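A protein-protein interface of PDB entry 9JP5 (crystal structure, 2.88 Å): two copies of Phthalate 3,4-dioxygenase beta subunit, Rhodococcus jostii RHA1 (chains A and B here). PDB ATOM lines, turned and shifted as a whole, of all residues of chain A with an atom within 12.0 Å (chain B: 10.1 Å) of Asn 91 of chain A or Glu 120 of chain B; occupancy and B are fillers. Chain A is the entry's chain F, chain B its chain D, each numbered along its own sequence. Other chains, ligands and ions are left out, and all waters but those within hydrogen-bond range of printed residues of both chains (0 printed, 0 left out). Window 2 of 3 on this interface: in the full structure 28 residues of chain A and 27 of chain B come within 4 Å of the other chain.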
ATOM      1  N   VAL A  86     -36.108 -28.563  -6.434  1.00  0.00           N
ATOM      2  CA  VAL A  86     -36.261 -27.134  -6.228  1.00  0.00           C
ATOM      3  C   VAL A  86     -35.228 -26.657  -5.191  1.00  0.00           C
ATOM      4  O   VAL A  86     -34.918 -27.337  -4.218  1.00  0.00           O
ATOM      5  CB  VAL A  86     -37.722 -26.805  -5.848  1.00  0.00           C
ATOM      6  CG1 VAL A  86     -38.705 -27.196  -6.942  1.00  0.00           C
ATOM      7  CG2 VAL A  86     -38.135 -27.472  -4.552  1.00  0.00           C
ATOM      8  N   THR A  87     -34.654 -25.484  -5.459  1.00  0.00           N
ATOM      9  CA  THR A  87     -33.703 -24.839  -4.576  1.00  0.00           C
ATOM     10  C   THR A  87     -34.448 -24.305  -3.359  1.00  0.00           C
ATOM     11  O   THR A  87     -35.443 -23.591  -3.515  1.00  0.00           O
ATOM     12  CB  THR A  87     -32.994 -23.700  -5.315  1.00  0.00           C
ATOM     13  OG1 THR A  87     -32.674 -24.159  -6.629  1.00  0.00           O
ATOM     14  CG2 THR A  87     -31.757 -23.214  -4.592  1.00  0.00           C
ATOM     15  N   THR A  88     -33.982 -24.676  -2.157  1.00  0.00           N
ATOM     16  CA  THR A  88     -34.672 -24.303  -0.931  1.00  0.00           C
ATOM     17  C   THR A  88     -33.687 -23.935   0.173  1.00  0.00           C
ATOM     18  O   THR A  88     -32.515 -24.298   0.157  1.00  0.00           O
ATOM     19  CB  THR A  88     -35.629 -25.390  -0.424  1.00  0.00           C
ATOM     20  OG1 THR A  88     -34.945 -26.636  -0.250  1.00  0.00           O
ATOM     21  CG2 THR A  88     -36.821 -25.595  -1.340  1.00  0.00           C
ATOM     22  N   ALA A  89     -34.211 -23.189   1.146  1.00  0.00           N
ATOM     23  CA  ALA A  89     -33.403 -22.694   2.243  1.00  0.00           C
ATOM     24  C   ALA A  89     -33.007 -23.876   3.128  1.00  0.00           C
ATOM     25  O   ALA A  89     -33.637 -24.927   3.048  1.00  0.00           O
ATOM     26  CB  ALA A  89     -34.175 -21.634   2.999  1.00  0.00           C
ATOM     27  N   LEU A  90     -32.012 -23.672   4.001  1.00  0.00           N
ATOM     28  CA  LEU A  90     -31.325 -24.773   4.652  1.00  0.00           C
ATOM     29  C   LEU A  90     -32.224 -25.583   5.588  1.00  0.00           C
ATOM     30  O   LEU A  90     -32.046 -26.802   5.686  1.00  0.00           O
ATOM     31  CB  LEU A  90     -30.103 -24.239   5.405  1.00  0.00           C
ATOM     32  CG  LEU A  90     -28.761 -24.464   4.707  1.00  0.00           C
ATOM     33  CD1 LEU A  90     -27.608 -24.045   5.626  1.00  0.00           C
ATOM     34  CD2 LEU A  90     -28.606 -25.921   4.234  1.00  0.00           C
ATOM     35  N   ASN A  91     -33.163 -24.949   6.304  1.00  0.00           N
ATOM     36  CA  ASN A  91     -33.930 -25.712   7.285  1.00  0.00           C
ATOM     37  C   ASN A  91     -35.390 -25.826   6.844  1.00  0.00           C
ATOM     38  O   ASN A  91     -36.281 -25.959   7.673  1.00  0.00           O
ATOM     39  CB  ASN A  91     -33.698 -25.166   8.699  1.00  0.00           C
ATOM     40  CG  ASN A  91     -32.320 -25.546   9.203  1.00  0.00           C
ATOM     41  OD1 ASN A  91     -32.109 -26.682   9.624  1.00  0.00           O
ATOM     42  ND2 ASN A  91     -31.367 -24.629   9.116  1.00  0.00           N
ATOM     43  N   SER A  92     -35.626 -25.873   5.532  1.00  0.00           N
ATOM     44  CA  SER A  92     -36.971 -25.957   4.996  1.00  0.00           C
ATOM     45  C   SER A  92     -37.499 -27.392   4.999  1.00  0.00           C
ATOM     46  O   SER A  92     -38.684 -27.597   4.747  1.00  0.00           O
ATOM     47  CB  SER A  92     -37.020 -25.367   3.611  1.00  0.00           C
ATOM     48  OG  SER A  92     -36.264 -26.151   2.711  1.00  0.00           O
ATOM     49  N   GLY A  93     -36.636 -28.385   5.228  1.00  0.00           N
ATOM     50  CA  GLY A  93     -37.095 -29.759   5.340  1.00  0.00           C
ATOM     51  C   GLY A  93     -37.575 -30.404   4.029  1.00  0.00           C
ATOM     52  O   GLY A  93     -38.283 -31.404   4.066  1.00  0.00           O
ATOM     53  N   PHE A  94     -37.193 -29.882   2.858  1.00  0.00           N
ATOM     54  CA  PHE A  94     -37.538 -30.517   1.592  1.00  0.00           C
ATOM     55  C   PHE A  94     -36.795 -29.817   0.458  1.00  0.00           C
ATOM     56  O   PHE A  94     -36.277 -28.713   0.642  1.00  0.00           O
ATOM     57  CB  PHE A  94     -39.033 -30.443   1.274  1.00  0.00           C
ATOM     58  CG  PHE A  94     -39.494 -29.079   0.833  1.00  0.00           C
ATOM     59  CD1 PHE A  94     -39.543 -28.020   1.727  1.00  0.00           C
ATOM     60  CD2 PHE A  94     -39.837 -28.846  -0.487  1.00  0.00           C
ATOM     61  CE1 PHE A  94     -39.951 -26.760   1.320  1.00  0.00           C
ATOM     62  CE2 PHE A  94     -40.232 -27.579  -0.897  1.00  0.00           C
ATOM     63  CZ  PHE A  94     -40.289 -26.535   0.008  1.00  0.00           C
ATOM     64  N   ASP A  95     -36.749 -30.477  -0.708  1.00  0.00           N
ATOM     65  CA  ASP A  95     -36.052 -29.930  -1.864  1.00  0.00           C
ATOM     66  C   ASP A  95     -36.583 -30.532  -3.170  1.00  0.00           C
ATOM     67  O   ASP A  95     -35.867 -30.648  -4.170  1.00  0.00           O
ATOM     68  CB  ASP A  95     -34.542 -30.100  -1.696  1.00  0.00           C
ATOM     69  CG  ASP A  95     -34.056 -31.532  -1.737  1.00  0.00           C
ATOM     70  OD1 ASP A  95     -34.895 -32.464  -1.579  1.00  0.00           O
ATOM     71  OD2 ASP A  95     -32.845 -31.691  -1.983  1.00  0.00           O
ATOM     72  N   THR A  96     -37.874 -30.864  -3.165  1.00  0.00           N
ATOM     73  CA  THR A  96     -38.542 -31.348  -4.353  1.00  0.00           C
ATOM     74  C   THR A  96     -39.914 -30.697  -4.419  1.00  0.00           C
ATOM     75  O   THR A  96     -40.468 -30.326  -3.382  1.00  0.00           O
ATOM     76  CB  THR A  96     -38.695 -32.868  -4.331  1.00  0.00           C
ATOM     77  OG1 THR A  96     -39.363 -33.143  -3.102  1.00  0.00           O
ATOM     78  CG2 THR A  96     -37.382 -33.609  -4.402  1.00  0.00           C
ATOM     79  N   GLN B  65     -22.708 -32.909   1.841  1.00  0.00           N
ATOM     80  CA  GLN B  65     -22.114 -31.823   2.605  1.00  0.00           C
ATOM     81  C   GLN B  65     -22.032 -32.178   4.085  1.00  0.00           C
ATOM     82  O   GLN B  65     -22.206 -31.300   4.926  1.00  0.00           O
ATOM     83  CB  GLN B  65     -22.898 -30.535   2.375  1.00  0.00           C
ATOM     84  CG  GLN B  65     -23.118 -30.272   0.893  1.00  0.00           C
ATOM     85  CD  GLN B  65     -23.546 -28.865   0.566  1.00  0.00           C
ATOM     86  OE1 GLN B  65     -24.481 -28.670  -0.207  1.00  0.00           O
ATOM     87  NE2 GLN B  65     -22.832 -27.884   1.107  1.00  0.00           N
ATOM     88  N   TYR B  67     -19.774 -32.381   6.267  1.00  0.00           N
ATOM     89  CA  TYR B  67     -18.388 -31.972   6.353  1.00  0.00           C
ATOM     90  C   TYR B  67     -17.793 -32.461   7.668  1.00  0.00           C
ATOM     91  O   TYR B  67     -16.598 -32.710   7.716  1.00  0.00           O
ATOM     92  CB  TYR B  67     -18.290 -30.469   6.061  1.00  0.00           C
ATOM     93  CG  TYR B  67     -18.690 -30.079   4.639  1.00  0.00           C
ATOM     94  CD1 TYR B  67     -18.226 -30.788   3.534  1.00  0.00           C
ATOM     95  CD2 TYR B  67     -19.500 -28.985   4.383  1.00  0.00           C
ATOM     96  CE1 TYR B  67     -18.562 -30.434   2.236  1.00  0.00           C
ATOM     97  CE2 TYR B  67     -19.831 -28.611   3.091  1.00  0.00           C
ATOM     98  CZ  TYR B  67     -19.370 -29.336   2.005  1.00  0.00           C
ATOM     99  OH  TYR B  67     -19.693 -28.971   0.718  1.00  0.00           O
ATOM    100  N   GLN B  68     -18.614 -32.642   8.713  1.00  0.00           N
ATOM    101  CA  GLN B  68     -18.102 -33.063  10.016  1.00  0.00           C
ATOM    102  C   GLN B  68     -17.648 -34.529   9.992  1.00  0.00           C
ATOM    103  O   GLN B  68     -16.530 -34.851  10.395  1.00  0.00           O
ATOM    104  CB  GLN B  68     -19.146 -32.834  11.108  1.00  0.00           C
ATOM    105  CG  GLN B  68     -18.966 -31.504  11.813  1.00  0.00           C
ATOM    106  CD  GLN B  68     -20.279 -30.887  12.220  1.00  0.00           C
ATOM    107  OE1 GLN B  68     -21.363 -31.340  11.848  1.00  0.00           O
ATOM    108  NE2 GLN B  68     -20.172 -29.814  12.985  1.00  0.00           N
ATOM    109  N   ARG B 113     -12.911 -23.955   8.346  1.00  0.00           N
ATOM    110  CA  ARG B 113     -13.688 -23.839   7.121  1.00  0.00           C
ATOM    111  C   ARG B 113     -15.009 -24.575   7.278  1.00  0.00           C
ATOM    112  O   ARG B 113     -16.039 -24.055   6.893  1.00  0.00           O
ATOM    113  CB  ARG B 113     -12.941 -24.374   5.892  1.00  0.00           C
ATOM    114  CG  ARG B 113     -11.873 -23.440   5.338  1.00  0.00           C
ATOM    115  CD  ARG B 113     -11.174 -24.060   4.152  1.00  0.00           C
ATOM    116  NE  ARG B 113      -9.991 -23.334   3.709  1.00  0.00           N
ATOM    117  CZ  ARG B 113      -9.998 -22.284   2.890  1.00  0.00           C
ATOM    118  NH1 ARG B 113     -11.135 -21.712   2.547  1.00  0.00           N
ATOM    119  NH2 ARG B 113      -8.863 -21.768   2.442  1.00  0.00           N
ATOM    120  N   VAL B 114     -14.960 -25.781   7.827  1.00  0.00           N
ATOM    121  CA  VAL B 114     -16.158 -26.570   8.040  1.00  0.00           C
ATOM    122  C   VAL B 114     -17.001 -25.951   9.157  1.00  0.00           C
ATOM    123  O   VAL B 114     -18.229 -25.951   9.088  1.00  0.00           O
ATOM    124  CB  VAL B 114     -15.771 -28.016   8.374  1.00  0.00           C
ATOM    125  CG1 VAL B 114     -16.962 -28.835   8.849  1.00  0.00           C
ATOM    126  CG2 VAL B 114     -15.087 -28.690   7.193  1.00  0.00           C
ATOM    127  N   ALA B 115     -16.337 -25.436  10.196  1.00  0.00           N
ATOM    128  CA  ALA B 115     -17.036 -24.801  11.301  1.00  0.00           C
ATOM    129  C   ALA B 115     -17.989 -23.716  10.785  1.00  0.00           C
ATOM    130  O   ALA B 115     -19.091 -23.527  11.313  1.00  0.00           O
ATOM    131  CB  ALA B 115     -16.020 -24.233  12.257  1.00  0.00           C
ATOM    132  N   ARG B 116     -17.525 -23.022   9.738  1.00  0.00           N
ATOM    133  CA  ARG B 116     -18.207 -21.912   9.093  1.00  0.00           C
ATOM    134  C   ARG B 116     -19.526 -22.338   8.453  1.00  0.00           C
ATOM    135  O   ARG B 116     -20.516 -21.614   8.569  1.00  0.00           O
ATOM    136  CB  ARG B 116     -17.300 -21.378   7.988  1.00  0.00           C
ATOM    137  CG  ARG B 116     -17.659 -19.986   7.515  1.00  0.00           C
ATOM    138  CD  ARG B 116     -17.537 -19.872   6.013  1.00  0.00           C
ATOM    139  NE  ARG B 116     -18.339 -18.737   5.640  1.00  0.00           N
ATOM    140  CZ  ARG B 116     -18.589 -18.377   4.403  1.00  0.00           C
ATOM    141  NH1 ARG B 116     -18.083 -19.052   3.383  1.00  0.00           N
ATOM    142  NH2 ARG B 116     -19.347 -17.320   4.209  1.00  0.00           N
ATOM    143  N   PHE B 117     -19.517 -23.472   7.735  1.00  0.00           N
ATOM    144  CA  PHE B 117     -20.736 -24.042   7.182  1.00  0.00           C
ATOM    145  C   PHE B 117     -21.643 -24.483   8.324  1.00  0.00           C
ATOM    146  O   PHE B 117     -22.860 -24.429   8.205  1.00  0.00           O
ATOM    147  CB  PHE B 117     -20.445 -25.223   6.249  1.00  0.00           C
ATOM    148  CG  PHE B 117     -19.685 -24.875   4.993  1.00  0.00           C
ATOM    149  CD1 PHE B 117     -20.329 -24.354   3.881  1.00  0.00           C
ATOM    150  CD2 PHE B 117     -18.307 -25.048   4.931  1.00  0.00           C
ATOM    151  CE1 PHE B 117     -19.607 -24.031   2.741  1.00  0.00           C
ATOM    152  CE2 PHE B 117     -17.588 -24.698   3.797  1.00  0.00           C
ATOM    153  CZ  PHE B 117     -18.239 -24.189   2.705  1.00  0.00           C
ATOM    154  N   VAL B 118     -21.044 -24.911   9.439  1.00  0.00           N
ATOM    155  CA  VAL B 118     -21.810 -25.388  10.580  1.00  0.00           C
ATOM    156  C   VAL B 118     -22.619 -24.256  11.212  1.00  0.00           C
ATOM    157  O   VAL B 118     -23.691 -24.543  11.729  1.00  0.00           O
ATOM    158  CB  VAL B 118     -20.909 -26.083  11.620  1.00  0.00           C
ATOM    159  CG1 VAL B 118     -21.629 -26.349  12.936  1.00  0.00           C
ATOM    160  CG2 VAL B 118     -20.338 -27.377  11.063  1.00  0.00           C
ATOM    161  N   THR B 119     -22.139 -22.998  11.172  1.00  0.00           N
ATOM    162  CA  THR B 119     -22.888 -21.870  11.732  1.00  0.00           C
ATOM    163  C   THR B 119     -24.233 -21.680  11.011  1.00  0.00           C
ATOM    164  O   THR B 119     -25.169 -21.147  11.581  1.00  0.00           O
ATOM    165  CB  THR B 119     -22.088 -20.548  11.748  1.00  0.00           C
ATOM    166  OG1 THR B 119     -22.074 -19.920  10.466  1.00  0.00           O
ATOM    167  CG2 THR B 119     -20.651 -20.688  12.199  1.00  0.00           C
ATOM    168  N   GLU B 120     -24.344 -22.098   9.750  1.00  0.00           N
ATOM    169  CA  GLU B 120     -25.505 -21.821   8.908  1.00  0.00           C
ATOM    170  C   GLU B 120     -25.626 -20.330   8.600  1.00  0.00           C
ATOM    171  O   GLU B 120     -26.714 -19.883   8.257  1.00  0.00           O
ATOM    172  CB  GLU B 120     -26.804 -22.333   9.534  1.00  0.00           C
ATOM    173  CG  GLU B 120     -26.826 -23.843   9.746  1.00  0.00           C
ATOM    174  CD  GLU B 120     -28.108 -24.429  10.331  1.00  0.00           C
ATOM    175  OE1 GLU B 120     -28.708 -25.291   9.680  1.00  0.00           O
ATOM    176  OE2 GLU B 120     -28.504 -24.033  11.447  1.00  0.00           O
ATOM    177  N   HIS B 121     -24.506 -19.592   8.698  1.00  0.00           N
ATOM    178  CA  HIS B 121     -24.431 -18.168   8.396  1.00  0.00           C
ATOM    179  C   HIS B 121     -23.448 -17.924   7.236  1.00  0.00           C
ATOM    180  O   HIS B 121     -22.988 -16.792   7.006  1.00  0.00           O
ATOM    181  CB  HIS B 121     -24.128 -17.395   9.688  1.00  0.00           C
ATOM    182  CG  HIS B 121     -25.227 -17.439  10.714  1.00  0.00           C
ATOM    183  ND1 HIS B 121     -26.533 -17.791  10.432  1.00  0.00           N
ATOM    184  CD2 HIS B 121     -25.213 -17.147  12.019  1.00  0.00           C
ATOM    185  CE1 HIS B 121     -27.266 -17.726  11.535  1.00  0.00           C
ATOM    186  NE2 HIS B 121     -26.479 -17.342  12.514  1.00  0.00           N
ATOM    187  N   ALA B 122     -23.143 -19.008   6.503  1.00  0.00           N
ATOM    188  CA  ALA B 122     -22.337 -18.955   5.299  1.00  0.00           C
ATOM    189  C   ALA B 122     -23.262 -18.737   4.111  1.00  0.00           C
ATOM    190  O   ALA B 122     -23.720 -19.692   3.499  1.00  0.00           O
ATOM    191  CB  ALA B 122     -21.564 -20.234   5.157  1.00  0.00           C
ATOM    192  N   TRP B 123     -23.497 -17.465   3.786  1.00  0.00           N
ATOM    193  CA  TRP B 123     -24.645 -17.051   3.000  1.00  0.00           C
ATOM    194  C   TRP B 123     -24.577 -17.615   1.582  1.00  0.00           C
ATOM    195  O   TRP B 123     -25.592 -17.919   0.976  1.00  0.00           O
ATOM    196  CB  TRP B 123     -24.717 -15.520   3.016  1.00  0.00           C
ATOM    197  CG  TRP B 123     -24.725 -14.899   4.401  1.00  0.00           C
ATOM    198  CD1 TRP B 123     -23.892 -13.923   4.876  1.00  0.00           C
ATOM    199  CD2 TRP B 123     -25.644 -15.192   5.484  1.00  0.00           C
ATOM    200  NE1 TRP B 123     -24.222 -13.584   6.159  1.00  0.00           N
ATOM    201  CE2 TRP B 123     -25.290 -14.341   6.557  1.00  0.00           C
ATOM    202  CE3 TRP B 123     -26.728 -16.078   5.649  1.00  0.00           C
ATOM    203  CZ2 TRP B 123     -25.986 -14.367   7.769  1.00  0.00           C
ATOM    204  CZ3 TRP B 123     -27.411 -16.100   6.850  1.00  0.00           C
ATOM    205  CH2 TRP B 123     -27.046 -15.249   7.893  1.00  0.00           C
ATOM    206  N   THR B 124     -23.368 -17.822   1.073  1.00  0.00           N
ATOM    207  CA  THR B 124     -23.189 -18.218  -0.311  1.00  0.00           C
ATOM    208  C   THR B 124     -23.620 -19.661  -0.541  1.00  0.00           C
ATOM    209  O   THR B 124     -23.657 -20.102  -1.685  1.00  0.00           O
ATOM    210  CB  THR B 124     -21.731 -18.044  -0.758  1.00  0.00           C
ATOM    211  OG1 THR B 124     -21.770 -17.967  -2.185  1.00  0.00           O
ATOM    212  CG2 THR B 124     -20.807 -19.146  -0.281  1.00  0.00           C
ATOM    213  N   GLU B 125     -23.904 -20.396   0.542  1.00  0.00           N
ATOM    214  CA  GLU B 125     -24.297 -21.797   0.455  1.00  0.00           C
ATOM    215  C   GLU B 125     -25.580 -22.060   1.247  1.00  0.00           C
ATOM    216  O   GLU B 125     -25.894 -23.209   1.584  1.00  0.00           O
ATOM    217  CB  GLU B 125     -23.130 -22.666   0.907  1.00  0.00           C
ATOM    218  CG  GLU B 125     -22.246 -23.082  -0.256  1.00  0.00           C
ATOM    219  CD  GLU B 125     -22.961 -23.885  -1.338  1.00  0.00           C
ATOM    220  OE1 GLU B 125     -22.743 -23.571  -2.530  1.00  0.00           O
ATOM    221  OE2 GLU B 125     -23.752 -24.815  -0.993  1.00  0.00           O
ATOM    222  N   ASP B 126     -26.338 -20.979   1.487  1.00  0.00           N
ATOM    223  CA  ASP B 126     -27.737 -21.101   1.867  1.00  0.00           C
ATOM    224  C   ASP B 126     -28.605 -20.221   0.967  1.00  0.00           C
ATOM    225  O   ASP B 126     -28.597 -19.004   1.087  1.00  0.00           O
ATOM    226  CB  ASP B 126     -27.927 -20.762   3.340  1.00  0.00           C
ATOM    227  CG  ASP B 126     -29.314 -21.103   3.832  1.00  0.00           C
ATOM    228  OD1 ASP B 126     -30.077 -21.628   3.014  1.00  0.00           O
ATOM    229  OD2 ASP B 126     -29.596 -20.846   5.017  1.00  0.00           O
ATOM    230  N   PRO B 127     -29.396 -20.773   0.027  1.00  0.00           N
ATOM    231  CA  PRO B 127     -29.528 -22.217  -0.197  1.00  0.00           C
ATOM    232  C   PRO B 127     -28.272 -22.978  -0.624  1.00  0.00           C
ATOM    233  O   PRO B 127     -27.363 -22.402  -1.225  1.00  0.00           O
ATOM    234  CB  PRO B 127     -30.500 -22.321  -1.384  1.00  0.00           C
ATOM    235  CG  PRO B 127     -31.256 -21.002  -1.384  1.00  0.00           C
ATOM    236  CD  PRO B 127     -30.250 -19.988  -0.874  1.00  0.00           C
ATOM    237  N   PRO B 128     -28.209 -24.309  -0.371  1.00  0.00           N
ATOM    238  CA  PRO B 128     -27.064 -25.125  -0.770  1.00  0.00           C
ATOM    239  C   PRO B 128     -26.991 -25.410  -2.263  1.00  0.00           C
ATOM    240  O   PRO B 128     -28.020 -25.609  -2.884  1.00  0.00           O
ATOM    241  CB  PRO B 128     -27.316 -26.469  -0.072  1.00  0.00           C
ATOM    242  CG  PRO B 128     -28.807 -26.542   0.082  1.00  0.00           C
ATOM    243  CD  PRO B 128     -29.251 -25.109   0.288  1.00  0.00           C
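Of chain B, only Glu 120 (2.8 Å) comes within 4 Å of Asn 91 of chain A. Ala 89 of chain A touches just one residue of chain B: Asp 126. Of chain B, only Asp 126 (3.0 Å) comes within 4 Å of Leu 90 of chain A. No residue of chain B comes within 4 Å of Ser 92 of chain A. No residue of chain A comes within 4 Å of Val 118 of chain B. No residue of chain A comes within 4 Å of Trp 123 of chain B. Asp 126 of chain B touches just these residues of chain A: Ala 89 and Leu 90. Of the printed residues of chain B, Thr 88 of chain A touches Pro 127 and Pro 128. Of the printed residues of chain A, Pro 127 of chain B touches Thr 87 and Thr 88. Printed residues of chain A within 4 Å of Pro 128 of chain B: Thr 88. Printed residues of chain B within 4 Å of Thr 87 of chain A: Pro 127. Ala 115 of chain B touches none of the printed residues of chain A. The nearest residue of chain B that does not touch Asn 91 of chain A is Asp 126 of chain B (5.6 Å). The nearest residue of chain A that does not touch Glu 120 of chain B is Leu 90 of chain A (4.2 Å). The nearest printed residue of chain A that does not touch Pro 127 of chain B is Ala 89 of chain A (4.5 Å).
CG2 of Thr 87 of chain A touches CB of Pro 127 of chain B (3.6 Å). Thr 88 of chain A touches Pro 127 of chain B. Pro 128 of chain B touches Thr 88 of chain A. Asp 126 of chain B touches Ala 89 of chain A (OD1 to CA, 3.6 Å).
Printed residues of chain B that touch a printed residue of chain A: Glu 120, Asp 126, Pro 127 and Pro 128. Hydrophobic or aromatic side chains of chain B that line the printed part of chain A: Pro 127 and Pro 128. Of the 11 printed residues of chain A, 5 touch a printed residue of chain B. Hydrophobic or aromatic side chains of chain A within 4 Å of the printed part of chain B: Leu 90. Among the printed residues, 6 pairs touch across the chains.
OE1 of Glu 120 of chain B lies within hydrogen-bond range of ND2 of Asn 91 of chain A (2.8 Å). The backbone NH of Leu 90 of chain A lies within hydrogen-bond range of the side-chain carboxylate of Asp 126 of chain B (3.0 Å).
No position is printed for both chains.
The side-chain hydroxyl of Thr 88 of chain A is in hydrogen-bond range of the side-chain hydroxyl of Ser 92 of chain A, 3.3 Å away. The side-chain hydroxyl (OG1) of Thr 88 of chain A is in hydrogen-bond range of the backbone carbonyl oxygen (O) of Phe 94 of chain A (2.6 Å). OG of Ser 92 of chain A is in hydrogen-bond range of O of Ala 89 of chain A, at 2.9 Å.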
